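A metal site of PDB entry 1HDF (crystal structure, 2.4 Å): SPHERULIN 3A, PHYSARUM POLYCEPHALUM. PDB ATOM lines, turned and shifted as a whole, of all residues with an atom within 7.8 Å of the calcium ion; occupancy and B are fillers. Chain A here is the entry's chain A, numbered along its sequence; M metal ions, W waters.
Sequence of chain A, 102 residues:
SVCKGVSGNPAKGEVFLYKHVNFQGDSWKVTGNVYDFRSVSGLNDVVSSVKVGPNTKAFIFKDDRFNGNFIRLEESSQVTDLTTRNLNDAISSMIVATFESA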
ATOM      1  N   TYR A  18      10.711 -32.172  -2.236  1.00  0.00           N
ATOM      2  CA  TYR A  18      11.727 -32.560  -1.258  1.00  0.00           C
ATOM      3  C   TYR A  18      12.560 -31.365  -0.839  1.00  0.00           C
ATOM      4  O   TYR A  18      12.939 -30.539  -1.670  1.00  0.00           O
ATOM      5  CB  TYR A  18      12.630 -33.642  -1.831  1.00  0.00           C
ATOM      6  CG  TYR A  18      11.894 -34.854  -2.364  1.00  0.00           C
ATOM      7  CD1 TYR A  18      11.263 -34.817  -3.604  1.00  0.00           C
ATOM      8  CD2 TYR A  18      11.831 -36.029  -1.621  1.00  0.00           C
ATOM      9  CE1 TYR A  18      10.581 -35.928  -4.088  1.00  0.00           C
ATOM     10  CE2 TYR A  18      11.163 -37.147  -2.097  1.00  0.00           C
ATOM     11  CZ  TYR A  18      10.531 -37.088  -3.331  1.00  0.00           C
ATOM     12  OH  TYR A  18       9.832 -38.187  -3.794  1.00  0.00           O
ATOM     13  N   LYS A  19      12.879 -31.289   0.448  1.00  0.00           N
ATOM     14  CA  LYS A  19      13.664 -30.174   0.971  1.00  0.00           C
ATOM     15  C   LYS A  19      15.118 -30.158   0.496  1.00  0.00           C
ATOM     16  O   LYS A  19      15.704 -29.089   0.318  1.00  0.00           O
ATOM     17  CB  LYS A  19      13.612 -30.179   2.513  1.00  0.00           C
ATOM     18  CG  LYS A  19      14.215 -28.938   3.144  1.00  0.00           C
ATOM     19  CD  LYS A  19      13.947 -28.906   4.633  1.00  0.00           C
ATOM     20  CE  LYS A  19      14.514 -27.641   5.257  1.00  0.00           C
ATOM     21  NZ  LYS A  19      14.195 -27.581   6.721  1.00  0.00           N
ATOM     22  N   HIS A  20      15.702 -31.332   0.295  1.00  0.00           N
ATOM     23  CA  HIS A  20      17.078 -31.382  -0.188  1.00  0.00           C
ATOM     24  C   HIS A  20      17.133 -31.927  -1.591  1.00  0.00           C
ATOM     25  O   HIS A  20      16.158 -32.490  -2.093  1.00  0.00           O
ATOM     26  CB  HIS A  20      17.945 -32.237   0.745  1.00  0.00           C
ATOM     27  CG  HIS A  20      18.060 -31.680   2.126  1.00  0.00           C
ATOM     28  ND1 HIS A  20      18.591 -32.399   3.180  1.00  0.00           N
ATOM     29  CD2 HIS A  20      17.691 -30.483   2.640  1.00  0.00           C
ATOM     30  CE1 HIS A  20      18.539 -31.667   4.275  1.00  0.00           C
ATOM     31  NE2 HIS A  20      17.993 -30.501   3.984  1.00  0.00           N
ATOM     32  N   VAL A  21      18.271 -31.750  -2.250  1.00  0.00           N
ATOM     33  CA  VAL A  21      18.429 -32.258  -3.602  1.00  0.00           C
ATOM     34  C   VAL A  21      18.415 -33.781  -3.570  1.00  0.00           C
ATOM     35  O   VAL A  21      18.449 -34.392  -2.507  1.00  0.00           O
ATOM     36  CB  VAL A  21      19.750 -31.768  -4.230  1.00  0.00           C
ATOM     37  CG1 VAL A  21      19.691 -30.269  -4.429  1.00  0.00           C
ATOM     38  CG2 VAL A  21      20.909 -32.139  -3.332  1.00  0.00           C
ATOM     39  N   GLN A  24      15.932 -35.951  -1.093  1.00  0.00           N
ATOM     40  CA  GLN A  24      16.236 -36.237   0.304  1.00  0.00           C
ATOM     41  C   GLN A  24      15.638 -35.170   1.239  1.00  0.00           C
ATOM     42  O   GLN A  24      15.219 -34.107   0.795  1.00  0.00           O
ATOM     43  CB  GLN A  24      17.740 -36.275   0.515  1.00  0.00           C
ATOM     44  CG  GLN A  24      18.470 -37.295  -0.337  1.00  0.00           C
ATOM     45  CD  GLN A  24      18.226 -38.718   0.128  1.00  0.00           C
ATOM     46  OE1 GLN A  24      18.493 -39.058   1.282  1.00  0.00           O
ATOM     47  NE2 GLN A  24      17.717 -39.553  -0.769  1.00  0.00           N
ATOM     48  N   ASP A  45      10.111 -21.574   0.329  1.00  0.00           N
ATOM     49  CA  ASP A  45      11.516 -21.390   0.017  1.00  0.00           C
ATOM     50  C   ASP A  45      12.512 -22.450   0.482  1.00  0.00           C
ATOM     51  O   ASP A  45      13.655 -22.105   0.783  1.00  0.00           O
ATOM     52  CB  ASP A  45      11.972 -20.019   0.537  1.00  0.00           C
ATOM     53  CG  ASP A  45      11.284 -18.867  -0.181  1.00  0.00           C
ATOM     54  OD1 ASP A  45      10.722 -19.097  -1.269  1.00  0.00           O
ATOM     55  OD2 ASP A  45      11.317 -17.729   0.335  1.00  0.00           O
ATOM     56  N   VAL A  46      12.122 -23.719   0.533  1.00  0.00           N
ATOM     57  CA  VAL A  46      13.059 -24.769   0.936  1.00  0.00           C
ATOM     58  C   VAL A  46      13.168 -25.934  -0.040  1.00  0.00           C
ATOM     59  O   VAL A  46      14.062 -26.766   0.090  1.00  0.00           O
ATOM     60  CB  VAL A  46      12.731 -25.363   2.333  1.00  0.00           C
ATOM     61  CG1 VAL A  46      12.587 -24.224   3.366  1.00  0.00           C
ATOM     62  CG2 VAL A  46      11.474 -26.217   2.262  1.00  0.00           C
ATOM     63  N   VAL A  47      12.266 -26.000  -1.012  1.00  0.00           N
ATOM     64  CA  VAL A  47      12.265 -27.087  -1.980  1.00  0.00           C
ATOM     65  C   VAL A  47      13.510 -27.114  -2.870  1.00  0.00           C
ATOM     66  O   VAL A  47      13.910 -26.096  -3.424  1.00  0.00           O
ATOM     67  CB  VAL A  47      10.992 -27.012  -2.877  1.00  0.00           C
ATOM     68  CG1 VAL A  47      10.992 -28.141  -3.899  1.00  0.00           C
ATOM     69  CG2 VAL A  47       9.758 -27.120  -2.000  1.00  0.00           C
ATOM     70  N   SER A  48      14.113 -28.292  -3.001  1.00  0.00           N
ATOM     71  CA  SER A  48      15.321 -28.431  -3.803  1.00  0.00           C
ATOM     72  C   SER A  48      15.233 -29.459  -4.922  1.00  0.00           C
ATOM     73  O   SER A  48      15.993 -29.390  -5.877  1.00  0.00           O
ATOM     74  CB  SER A  48      16.499 -28.745  -2.891  1.00  0.00           C
ATOM     75  OG  SER A  48      16.702 -27.669  -1.989  1.00  0.00           O
ATOM     76  N   SER A  49      14.311 -30.427  -4.793  1.00  0.00           N
ATOM     77  CA  SER A  49      14.115 -31.462  -5.812  1.00  0.00           C
ATOM     78  C   SER A  49      12.618 -31.764  -5.977  1.00  0.00           C
ATOM     79  O   SER A  49      11.834 -31.583  -5.043  1.00  0.00           O
ATOM     80  CB  SER A  49      14.883 -32.748  -5.472  1.00  0.00           C
ATOM     81  OG  SER A  49      14.409 -33.331  -4.274  1.00  0.00           O
ATOM     82  N   LEU A  82      17.022 -28.111  -8.085  1.00  0.00           N
ATOM     83  CA  LEU A  82      16.323 -26.962  -8.652  1.00  0.00           C
ATOM     84  C   LEU A  82      17.195 -25.765  -8.991  1.00  0.00           C
ATOM     85  O   LEU A  82      16.722 -24.806  -9.609  1.00  0.00           O
ATOM     86  CB  LEU A  82      15.181 -26.528  -7.713  1.00  0.00           C
ATOM     87  CG  LEU A  82      13.899 -27.367  -7.793  1.00  0.00           C
ATOM     88  CD1 LEU A  82      12.926 -26.957  -6.699  1.00  0.00           C
ATOM     89  CD2 LEU A  82      13.272 -27.177  -9.154  1.00  0.00           C
ATOM     90  N   ASN A  88      15.994 -22.936  -6.733  1.00  0.00           N
ATOM     91  CA  ASN A  88      16.301 -23.646  -5.501  1.00  0.00           C
ATOM     92  C   ASN A  88      15.883 -22.780  -4.319  1.00  0.00           C
ATOM     93  O   ASN A  88      16.067 -21.558  -4.342  1.00  0.00           O
ATOM     94  CB  ASN A  88      17.798 -23.949  -5.427  1.00  0.00           C
ATOM     95  CG  ASN A  88      18.161 -24.882  -4.272  1.00  0.00           C
ATOM     96  OD1 ASN A  88      19.246 -24.782  -3.699  1.00  0.00           O
ATOM     97  ND2 ASN A  88      17.247 -25.786  -3.929  1.00  0.00           N
ATOM     98  N   ASP A  89      15.306 -23.402  -3.288  1.00  0.00           N
ATOM     99  CA  ASP A  89      14.845 -22.685  -2.093  1.00  0.00           C
ATOM    100  C   ASP A  89      14.155 -21.367  -2.437  1.00  0.00           C
ATOM    101  O   ASP A  89      14.502 -20.335  -1.876  1.00  0.00           O
ATOM    102  CB  ASP A  89      16.025 -22.385  -1.157  1.00  0.00           C
ATOM    103  CG  ASP A  89      16.756 -23.635  -0.711  1.00  0.00           C
ATOM    104  OD1 ASP A  89      16.108 -24.690  -0.564  1.00  0.00           O
ATOM    105  OD2 ASP A  89      17.990 -23.560  -0.493  1.00  0.00           O
ATOM    106  N   ALA A  90      13.186 -21.397  -3.329  1.00  0.00           N
ATOM    107  CA  ALA A  90      12.505 -20.157  -3.710  1.00  0.00           C
ATOM    108  C   ALA A  90      11.057 -20.297  -4.135  1.00  0.00           C
ATOM    109  O   ALA A  90      10.363 -19.285  -4.302  1.00  0.00           O
ATOM    110  CB  ALA A  90      13.297 -19.472  -4.806  1.00  0.00           C
HETATM  111 CA    CA M   1      16.297 -26.876   0.124  1.00  0.00          CA
HETATM  112  O   HOH W   1      18.920 -26.760   0.266  1.00  0.00           O
HETATM  113  O   HOH W   2      16.323 -25.946   2.430  1.00  0.00           O
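The side-chain hydroxyl (OG) of Ser 48 sits close to the side-chain amide nitrogen (ND2) of Asn 88 (2.8 Å).
The backbone NH (N) of Ser 48 lies within hydrogen-bond range of the backbone carbonyl oxygen (O) of Tyr 18, at 2.9 Å.
The backbone carbonyl oxygen (O) of Ser 48 sits at hydrogen-bond distance from the backbone NH (N) of Leu 82 (2.8 Å).
The backbone NH (N) of Asp 89 lies within hydrogen-bond range of the backbone carbonyl oxygen (O) of Val 47, 3.0 Å away.
Within 4 Å of the calcium ion: Lys 19, Val 46, Ser 48 and Asp 89.
The calcium ion is bound by the backbone carbonyl oxygen of Val 46 (2.2 Å), the side-chain hydroxyl of Ser 48 (2.3 Å), the backbone carbonyl oxygen of Lys 19 (2.3 Å), the side-chain carboxylate of Asp 89 (2.3 Å), water W2 (2.5 Å) and water W1 (2.6 Å).
The calcium ion has six donor atoms within binding distance.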
